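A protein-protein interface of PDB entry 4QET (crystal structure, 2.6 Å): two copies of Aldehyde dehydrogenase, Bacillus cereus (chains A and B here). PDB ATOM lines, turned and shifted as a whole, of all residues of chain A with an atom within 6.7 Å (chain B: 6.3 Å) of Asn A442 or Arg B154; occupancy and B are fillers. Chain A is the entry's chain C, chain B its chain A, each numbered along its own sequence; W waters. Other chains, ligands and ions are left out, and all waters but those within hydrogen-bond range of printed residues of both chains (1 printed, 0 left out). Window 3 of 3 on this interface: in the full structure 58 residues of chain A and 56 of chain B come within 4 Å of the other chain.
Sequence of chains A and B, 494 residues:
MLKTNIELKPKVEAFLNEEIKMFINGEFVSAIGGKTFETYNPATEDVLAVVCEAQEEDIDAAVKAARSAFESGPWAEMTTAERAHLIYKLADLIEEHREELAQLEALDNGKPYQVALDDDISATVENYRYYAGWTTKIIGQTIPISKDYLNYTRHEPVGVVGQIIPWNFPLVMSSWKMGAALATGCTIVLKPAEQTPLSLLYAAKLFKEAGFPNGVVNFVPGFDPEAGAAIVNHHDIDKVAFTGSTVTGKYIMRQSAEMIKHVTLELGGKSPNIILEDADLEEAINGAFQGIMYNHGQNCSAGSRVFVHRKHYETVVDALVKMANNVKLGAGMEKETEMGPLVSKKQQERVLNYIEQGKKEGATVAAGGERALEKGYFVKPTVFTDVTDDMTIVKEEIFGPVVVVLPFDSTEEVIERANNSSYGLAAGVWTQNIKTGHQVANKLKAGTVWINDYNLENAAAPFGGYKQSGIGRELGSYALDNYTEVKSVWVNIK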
ATOM      1  N   THR A 436       3.115   2.373   0.861  1.00  0.00           N
ATOM      2  CA  THR A 436       3.736   3.420   1.601  1.00  0.00           C
ATOM      3  C   THR A 436       4.142   4.610   0.744  1.00  0.00           C
ATOM      4  O   THR A 436       4.030   5.744   1.181  1.00  0.00           O
ATOM      5  CB  THR A 436       4.988   2.897   2.329  1.00  0.00           C
ATOM      6  OG1 THR A 436       4.658   1.670   2.969  1.00  0.00           O
ATOM      7  CG2 THR A 436       5.452   3.930   3.405  1.00  0.00           C
ATOM      8  N   GLY A 437       4.636   4.349  -0.463  1.00  0.00           N
ATOM      9  CA  GLY A 437       5.157   5.393  -1.298  1.00  0.00           C
ATOM     10  C   GLY A 437       4.037   6.354  -1.614  1.00  0.00           C
ATOM     11  O   GLY A 437       4.203   7.582  -1.481  1.00  0.00           O
ATOM     12  N   HIS A 438       2.884   5.819  -2.002  1.00  0.00           N
ATOM     13  CA  HIS A 438       1.746   6.667  -2.298  1.00  0.00           C
ATOM     14  C   HIS A 438       1.103   7.289  -1.031  1.00  0.00           C
ATOM     15  O   HIS A 438       0.846   8.512  -0.985  1.00  0.00           O
ATOM     16  CB  HIS A 438       0.749   5.890  -3.131  1.00  0.00           C
ATOM     17  CG  HIS A 438       1.188   5.732  -4.545  1.00  0.00           C
ATOM     18  ND1 HIS A 438       1.407   4.497  -5.139  1.00  0.00           N
ATOM     19  CD2 HIS A 438       1.482   6.668  -5.482  1.00  0.00           C
ATOM     20  CE1 HIS A 438       1.804   4.686  -6.387  1.00  0.00           C
ATOM     21  NE2 HIS A 438       1.854   5.996  -6.620  1.00  0.00           N
ATOM     22  N   GLN A 439       0.903   6.471   0.005  1.00  0.00           N
ATOM     23  CA  GLN A 439       0.420   7.002   1.291  1.00  0.00           C
ATOM     24  C   GLN A 439       1.233   8.202   1.755  1.00  0.00           C
ATOM     25  O   GLN A 439       0.673   9.261   2.020  1.00  0.00           O
ATOM     26  CB  GLN A 439       0.380   5.951   2.402  1.00  0.00           C
ATOM     27  CG  GLN A 439      -0.804   4.996   2.337  1.00  0.00           C
ATOM     28  CD  GLN A 439      -0.528   3.678   3.058  1.00  0.00           C
ATOM     29  OE1 GLN A 439       0.406   3.587   3.838  1.00  0.00           O
ATOM     30  NE2 GLN A 439      -1.310   2.646   2.760  1.00  0.00           N
ATOM     31  N   VAL A 440       2.546   8.044   1.812  1.00  0.00           N
ATOM     32  CA  VAL A 440       3.410   9.093   2.333  1.00  0.00           C
ATOM     33  C   VAL A 440       3.388  10.301   1.445  1.00  0.00           C
ATOM     34  O   VAL A 440       3.213  11.420   1.974  1.00  0.00           O
ATOM     35  CB  VAL A 440       4.850   8.623   2.603  1.00  0.00           C
ATOM     36  CG1 VAL A 440       5.742   9.777   3.050  1.00  0.00           C
ATOM     37  CG2 VAL A 440       4.835   7.549   3.674  1.00  0.00           C
ATOM     38  N   ALA A 441       3.499  10.107   0.124  1.00  0.00           N
ATOM     39  CA  ALA A 441       3.446  11.258  -0.796  1.00  0.00           C
ATOM     40  C   ALA A 441       2.113  12.023  -0.723  1.00  0.00           C
ATOM     41  O   ALA A 441       2.094  13.252  -0.881  1.00  0.00           O
ATOM     42  CB  ALA A 441       3.727  10.845  -2.209  1.00  0.00           C
ATOM     43  N   ASN A 442       1.008  11.321  -0.462  1.00  0.00           N
ATOM     44  CA  ASN A 442      -0.300  11.997  -0.304  1.00  0.00           C
ATOM     45  C   ASN A 442      -0.400  12.917   0.891  1.00  0.00           C
ATOM     46  O   ASN A 442      -1.080  13.951   0.843  1.00  0.00           O
ATOM     47  CB  ASN A 442      -1.443  11.003  -0.213  1.00  0.00           C
ATOM     48  CG  ASN A 442      -1.798  10.389  -1.551  1.00  0.00           C
ATOM     49  OD1 ASN A 442      -2.496   9.392  -1.589  1.00  0.00           O
ATOM     50  ND2 ASN A 442      -1.320  10.977  -2.648  1.00  0.00           N
ATOM     51  N   LYS A 443       0.292  12.547   1.956  1.00  0.00           N
ATOM     52  CA  LYS A 443       0.258  13.323   3.203  1.00  0.00           C
ATOM     53  C   LYS A 443       1.356  14.387   3.363  1.00  0.00           C
ATOM     54  O   LYS A 443       1.242  15.199   4.240  1.00  0.00           O
ATOM     55  CB  LYS A 443       0.279  12.394   4.410  1.00  0.00           C
ATOM     56  CG  LYS A 443      -0.913  11.465   4.468  1.00  0.00           C
ATOM     57  CD  LYS A 443      -1.040  10.817   5.838  1.00  0.00           C
ATOM     58  CE  LYS A 443      -1.115   9.295   5.741  1.00  0.00           C
ATOM     59  NZ  LYS A 443      -2.337   8.863   5.006  1.00  0.00           N
ATOM     60  N   LEU A 444       2.427  14.377   2.567  1.00  0.00           N
ATOM     61  CA  LEU A 444       3.435  15.475   2.631  1.00  0.00           C
ATOM     62  C   LEU A 444       2.884  16.783   2.065  1.00  0.00           C
ATOM     63  O   LEU A 444       2.255  16.780   1.005  1.00  0.00           O
ATOM     64  CB  LEU A 444       4.763  15.114   1.945  1.00  0.00           C
ATOM     65  CG  LEU A 444       5.459  13.957   2.665  1.00  0.00           C
ATOM     66  CD1 LEU A 444       6.581  13.369   1.839  1.00  0.00           C
ATOM     67  CD2 LEU A 444       5.943  14.359   4.059  1.00  0.00           C
ATOM     68  N   LYS A 445       3.131  17.894   2.749  1.00  0.00           N
ATOM     69  CA  LYS A 445       2.610  19.144   2.263  1.00  0.00           C
ATOM     70  C   LYS A 445       3.640  19.863   1.423  1.00  0.00           C
ATOM     71  O   LYS A 445       4.324  20.765   1.907  1.00  0.00           O
ATOM     72  CB  LYS A 445       2.015  19.980   3.415  1.00  0.00           C
ATOM     73  CG  LYS A 445       0.541  19.649   3.653  1.00  0.00           C
ATOM     74  CD  LYS A 445       0.182  19.638   5.131  1.00  0.00           C
ATOM     75  CE  LYS A 445      -0.799  20.750   5.513  1.00  0.00           C
ATOM     76  NZ  LYS A 445      -2.151  20.243   5.873  1.00  0.00           N
ATOM     77  N   VAL A 449       6.658  15.968  -5.138  1.00  0.00           N
ATOM     78  CA  VAL A 449       7.132  14.855  -4.338  1.00  0.00           C
ATOM     79  C   VAL A 449       7.786  13.826  -5.245  1.00  0.00           C
ATOM     80  O   VAL A 449       7.174  13.341  -6.200  1.00  0.00           O
ATOM     81  CB  VAL A 449       5.998  14.127  -3.597  1.00  0.00           C
ATOM     82  CG1 VAL A 449       6.580  12.916  -2.843  1.00  0.00           C
ATOM     83  CG2 VAL A 449       5.231  15.069  -2.673  1.00  0.00           C
ATOM     84  N   TYR A 466       3.578  24.875  -1.495  1.00  0.00           N
ATOM     85  CA  TYR A 466       2.544  25.062  -0.438  1.00  0.00           C
ATOM     86  C   TYR A 466       3.032  26.115   0.575  1.00  0.00           C
ATOM     87  O   TYR A 466       4.213  26.488   0.548  1.00  0.00           O
ATOM     88  CB  TYR A 466       2.320  23.743   0.340  1.00  0.00           C
ATOM     89  CG  TYR A 466       1.559  22.617  -0.359  1.00  0.00           C
ATOM     90  CD1 TYR A 466       1.886  22.230  -1.650  1.00  0.00           C
ATOM     91  CD2 TYR A 466       0.521  21.934   0.298  1.00  0.00           C
ATOM     92  CE1 TYR A 466       1.205  21.233  -2.290  1.00  0.00           C
ATOM     93  CE2 TYR A 466      -0.151  20.895  -0.324  1.00  0.00           C
ATOM     94  CZ  TYR A 466       0.207  20.539  -1.636  1.00  0.00           C
ATOM     95  OH  TYR A 466      -0.435  19.497  -2.330  1.00  0.00           O
ATOM     96  N   TYR A 478      -0.114  24.402 -16.123  1.00  0.00           N
ATOM     97  CA  TYR A 478      -0.530  25.256 -15.000  1.00  0.00           C
ATOM     98  C   TYR A 478      -0.008  26.690 -15.099  1.00  0.00           C
ATOM     99  O   TYR A 478      -0.759  27.643 -14.921  1.00  0.00           O
ATOM    100  CB  TYR A 478      -0.132  24.596 -13.644  1.00  0.00           C
ATOM    101  CG  TYR A 478      -0.849  23.250 -13.419  1.00  0.00           C
ATOM    102  CD1 TYR A 478      -2.100  23.205 -12.782  1.00  0.00           C
ATOM    103  CD2 TYR A 478      -0.319  22.039 -13.934  1.00  0.00           C
ATOM    104  CE1 TYR A 478      -2.779  22.016 -12.629  1.00  0.00           C
ATOM    105  CE2 TYR A 478      -0.991  20.833 -13.777  1.00  0.00           C
ATOM    106  CZ  TYR A 478      -2.221  20.829 -13.109  1.00  0.00           C
ATOM    107  OH  TYR A 478      -2.935  19.660 -12.959  1.00  0.00           O
ATOM    108  N   GLY B 140      -6.869  15.697 -11.721  1.00  0.00           N
ATOM    109  CA  GLY B 140      -5.527  16.194 -11.930  1.00  0.00           C
ATOM    110  C   GLY B 140      -5.080  15.552 -13.228  1.00  0.00           C
ATOM    111  O   GLY B 140      -5.920  15.019 -13.936  1.00  0.00           O
ATOM    112  N   GLN B 141      -3.764  15.532 -13.504  1.00  0.00           N
ATOM    113  CA  GLN B 141      -3.238  15.150 -14.818  1.00  0.00           C
ATOM    114  C   GLN B 141      -2.345  13.945 -14.687  1.00  0.00           C
ATOM    115  O   GLN B 141      -1.710  13.769 -13.638  1.00  0.00           O
ATOM    116  CB  GLN B 141      -2.397  16.280 -15.409  1.00  0.00           C
ATOM    117  CG  GLN B 141      -3.091  17.644 -15.551  1.00  0.00           C
ATOM    118  CD  GLN B 141      -2.255  18.636 -16.359  1.00  0.00           C
ATOM    119  OE1 GLN B 141      -1.052  18.411 -16.600  1.00  0.00           O
ATOM    120  NE2 GLN B 141      -2.889  19.700 -16.831  1.00  0.00           N
ATOM    121  N   TYR B 152       2.274  12.332 -12.234  1.00  0.00           N
ATOM    122  CA  TYR B 152       0.888  12.763 -12.091  1.00  0.00           C
ATOM    123  C   TYR B 152       0.729  13.922 -11.111  1.00  0.00           C
ATOM    124  O   TYR B 152       1.590  14.139 -10.221  1.00  0.00           O
ATOM    125  CB  TYR B 152      -0.014  11.591 -11.690  1.00  0.00           C
ATOM    126  CG  TYR B 152       0.186  11.038 -10.288  1.00  0.00           C
ATOM    127  CD1 TYR B 152      -0.616  11.442  -9.230  1.00  0.00           C
ATOM    128  CD2 TYR B 152       1.160  10.062 -10.025  1.00  0.00           C
ATOM    129  CE1 TYR B 152      -0.449  10.887  -7.939  1.00  0.00           C
ATOM    130  CE2 TYR B 152       1.333   9.493  -8.753  1.00  0.00           C
ATOM    131  CZ  TYR B 152       0.533   9.923  -7.720  1.00  0.00           C
ATOM    132  OH  TYR B 152       0.707   9.379  -6.488  1.00  0.00           O
ATOM    133  N   THR B 153      -0.364  14.664 -11.271  1.00  0.00           N
ATOM    134  CA  THR B 153      -0.640  15.781 -10.361  1.00  0.00           C
ATOM    135  C   THR B 153      -1.870  15.435  -9.559  1.00  0.00           C
ATOM    136  O   THR B 153      -2.779  14.800 -10.089  1.00  0.00           O
ATOM    137  CB  THR B 153      -0.832  17.144 -11.118  1.00  0.00           C
ATOM    138  OG1 THR B 153      -2.003  17.079 -11.946  1.00  0.00           O
ATOM    139  CG2 THR B 153       0.403  17.492 -12.000  1.00  0.00           C
ATOM    140  N   ARG B 154      -1.904  15.836  -8.289  1.00  0.00           N
ATOM    141  CA  ARG B 154      -3.139  15.814  -7.480  1.00  0.00           C
ATOM    142  C   ARG B 154      -3.649  17.205  -7.231  1.00  0.00           C
ATOM    143  O   ARG B 154      -2.860  18.107  -6.944  1.00  0.00           O
ATOM    144  CB  ARG B 154      -2.863  15.227  -6.125  1.00  0.00           C
ATOM    145  CG  ARG B 154      -3.040  13.731  -6.067  1.00  0.00           C
ATOM    146  CD  ARG B 154      -2.238  13.143  -4.918  1.00  0.00           C
ATOM    147  NE  ARG B 154      -2.606  13.598  -3.576  1.00  0.00           N
ATOM    148  CZ  ARG B 154      -3.670  13.190  -2.873  1.00  0.00           C
ATOM    149  NH1 ARG B 154      -4.545  12.350  -3.389  1.00  0.00           N
ATOM    150  NH2 ARG B 154      -3.856  13.645  -1.635  1.00  0.00           N
ATOM    151  N   HIS B 155      -4.949  17.409  -7.318  1.00  0.00           N
ATOM    152  CA  HIS B 155      -5.498  18.703  -6.914  1.00  0.00           C
ATOM    153  C   HIS B 155      -6.046  18.568  -5.489  1.00  0.00           C
ATOM    154  O   HIS B 155      -7.168  18.146  -5.328  1.00  0.00           O
ATOM    155  CB  HIS B 155      -6.563  19.222  -7.906  1.00  0.00           C
ATOM    156  CG  HIS B 155      -6.025  19.537  -9.273  1.00  0.00           C
ATOM    157  ND1 HIS B 155      -6.752  20.228 -10.217  1.00  0.00           N
ATOM    158  CD2 HIS B 155      -4.830  19.261  -9.858  1.00  0.00           C
ATOM    159  CE1 HIS B 155      -6.043  20.347 -11.330  1.00  0.00           C
ATOM    160  NE2 HIS B 155      -4.873  19.768 -11.142  1.00  0.00           N
ATOM    161  N   GLU B 156      -5.236  18.900  -4.478  1.00  0.00           N
ATOM    162  CA  GLU B 156      -5.593  18.733  -3.078  1.00  0.00           C
ATOM    163  C   GLU B 156      -6.273  19.969  -2.549  1.00  0.00           C
ATOM    164  O   GLU B 156      -5.932  21.075  -2.999  1.00  0.00           O
ATOM    165  CB  GLU B 156      -4.341  18.484  -2.241  1.00  0.00           C
ATOM    166  CG  GLU B 156      -3.638  17.187  -2.599  1.00  0.00           C
ATOM    167  CD  GLU B 156      -2.431  16.870  -1.733  1.00  0.00           C
ATOM    168  OE1 GLU B 156      -2.085  17.631  -0.782  1.00  0.00           O
ATOM    169  OE2 GLU B 156      -1.824  15.824  -2.012  1.00  0.00           O
ATOM    170  N   THR B 484      -7.455  24.897  -4.255  1.00  0.00           N
ATOM    171  CA  THR B 484      -6.669  23.726  -4.544  1.00  0.00           C
ATOM    172  C   THR B 484      -5.197  24.054  -4.415  1.00  0.00           C
ATOM    173  O   THR B 484      -4.793  25.156  -4.739  1.00  0.00           O
ATOM    174  CB  THR B 484      -7.088  23.249  -5.962  1.00  0.00           C
ATOM    175  OG1 THR B 484      -8.019  22.179  -5.808  1.00  0.00           O
ATOM    176  CG2 THR B 484      -5.933  22.815  -6.873  1.00  0.00           C
ATOM    177  N   GLU B 485      -4.393  23.135  -3.903  1.00  0.00           N
ATOM    178  CA  GLU B 485      -2.925  23.180  -4.133  1.00  0.00           C
ATOM    179  C   GLU B 485      -2.601  22.076  -5.092  1.00  0.00           C
ATOM    180  O   GLU B 485      -3.078  20.931  -4.907  1.00  0.00           O
ATOM    181  CB  GLU B 485      -2.092  22.930  -2.858  1.00  0.00           C
ATOM    182  CG  GLU B 485      -2.039  24.104  -1.896  1.00  0.00           C
ATOM    183  CD  GLU B 485      -1.089  25.199  -2.351  1.00  0.00           C
ATOM    184  OE1 GLU B 485      -1.073  26.256  -1.691  1.00  0.00           O
ATOM    185  OE2 GLU B 485      -0.347  25.001  -3.351  1.00  0.00           O
ATOM    186  N   VAL B 486      -1.795  22.407  -6.106  1.00  0.00           N
ATOM    187  CA  VAL B 486      -1.290  21.419  -7.103  1.00  0.00           C
ATOM    188  C   VAL B 486      -0.026  20.696  -6.619  1.00  0.00           C
ATOM    189  O   VAL B 486       1.026  21.342  -6.387  1.00  0.00           O
ATOM    190  CB  VAL B 486      -1.081  22.061  -8.491  1.00  0.00           C
ATOM    191  CG1 VAL B 486      -0.650  21.013  -9.508  1.00  0.00           C
ATOM    192  CG2 VAL B 486      -2.398  22.704  -8.955  1.00  0.00           C
ATOM    193  N   LYS B 487      -0.151  19.373  -6.411  1.00  0.00           N
ATOM    194  CA  LYS B 487       0.995  18.537  -6.035  1.00  0.00           C
ATOM    195  C   LYS B 487       1.342  17.697  -7.247  1.00  0.00           C
ATOM    196  O   LYS B 487       0.512  16.945  -7.736  1.00  0.00           O
ATOM    197  CB  LYS B 487       0.677  17.633  -4.844  1.00  0.00           C
ATOM    198  CG  LYS B 487       1.749  16.581  -4.539  1.00  0.00           C
ATOM    199  CD  LYS B 487       1.460  15.735  -3.314  1.00  0.00           C
ATOM    200  CE  LYS B 487       1.218  16.580  -2.062  1.00  0.00           C
ATOM    201  NZ  LYS B 487       0.845  15.693  -0.901  1.00  0.00           N
ATOM    202  N   SER B 488       2.566  17.848  -7.731  1.00  0.00           N
ATOM    203  CA  SER B 488       3.123  17.059  -8.810  1.00  0.00           C
ATOM    204  C   SER B 488       4.016  15.924  -8.287  1.00  0.00           C
ATOM    205  O   SER B 488       5.035  16.178  -7.668  1.00  0.00           O
ATOM    206  CB  SER B 488       3.955  17.935  -9.691  1.00  0.00           C
ATOM    207  OG  SER B 488       4.946  17.112 -10.241  1.00  0.00           O
ATOM    208  N   VAL B 489       3.606  14.684  -8.554  1.00  0.00           N
ATOM    209  CA  VAL B 489       4.215  13.486  -8.024  1.00  0.00           C
ATOM    210  C   VAL B 489       5.031  12.796  -9.122  1.00  0.00           C
ATOM    211  O   VAL B 489       4.557  12.605 -10.248  1.00  0.00           O
ATOM    212  CB  VAL B 489       3.129  12.518  -7.451  1.00  0.00           C
ATOM    213  CG1 VAL B 489       3.752  11.204  -6.957  1.00  0.00           C
ATOM    214  CG2 VAL B 489       2.408  13.212  -6.325  1.00  0.00           C
HETATM  215  O   HOH W   1      -1.334   9.607  -4.686  1.00  0.00           O
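Hydrophobic or aromatic side chains of chain A within 4 Å of the printed part of chain B: His A438, Val A449, Tyr A466 and Tyr A478.
Among the printed residues, 16 pairs touch across the chains.
Among the printed residues, no Asp or Glu carboxylate lies within 4 Å of a Lys or Arg side-chain nitrogen of the other chain.
No position is printed for both chains.
Among the printed residues, merely in contact across the chains: His A438 with Tyr B152 (3.0 Å), Tyr A478 with Gln B141 (3.3 Å), Tyr A466 with Lys B487 (3.3 Å), Val A449 with Val B489 (3.5 Å), Tyr A466 with Glu B485 (3.5 Å), Tyr A478 with Val B486 (3.8 Å) and Val A449 with Lys B487 (3.9 Å).
The backbone carbonyl oxygen of Ser B488 sits at hydrogen-bond distance from the backbone NH of Val A449 (3.0 Å).
NZ of Lys B487 lies within hydrogen-bond range of O of Asn A442 (3.1 Å).
The guanidinium group (NE) of Arg B154 lies close to the side-chain amide nitrogen (ND2) of Asn A442 (3.1 Å).
O of Asn A442 sits close to OE2 of Glu B156, at 3.5 Å.
NZ of Lys B487 lies within hydrogen-bond range of O of Ala A441, 2.7 Å away.
NE2 of His B155 sits at hydrogen-bond distance from OH of Tyr A478.
The side-chain hydroxyl of Tyr A478 sits at hydrogen-bond distance from the side-chain hydroxyl of Thr B153 (2.9 Å).
O of Leu A444 lies within hydrogen-bond range of NZ of Lys B487 (2.6 Å).
OH of Tyr A466 lies within hydrogen-bond range of OE1 of Glu B156 (2.9 Å).
Printed residues of chain B within 4 Å of His A438: Tyr B152 (3.0 Å).
Asn A442 touches three residues of chain B.
Of the printed residues of chain A, Tyr B152 touches His A438 (3.0 Å).
Of the printed residues of chain A, Thr B153 touches Tyr A478 (2.9 Å).
Printed residues of chain A within 4 Å of Val B489: Val A449 (3.5 Å).
The nearest residue of chain A that does not touch Arg B154 is Tyr A466 (5.4 Å).
N of Gln B141 lies within hydrogen-bond range of OG1 of Thr B153 (2.8 Å).
The side-chain carboxylate of Glu B156 is in salt-bridge range of the side-chain amino group of Lys B487 (2.9 Å).
The backbone NH (N) of Arg B154 lies within hydrogen-bond range of the backbone carbonyl oxygen (O) of Lys B487 (2.7 Å).
N of Glu B485 sits at hydrogen-bond distance from O of Glu B156, at 2.7 Å.
O of Tyr B152 is in hydrogen-bond range of N of Val B489, at 2.7 Å.
OE2 of Glu B156 is in salt-bridge range of NE of Arg B154 (2.8 Å).
Water W1 lies within hydrogen-bond range of ND2 of Asn A442 (2.5 Å) and OH of Tyr B152 (2.7 Å).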
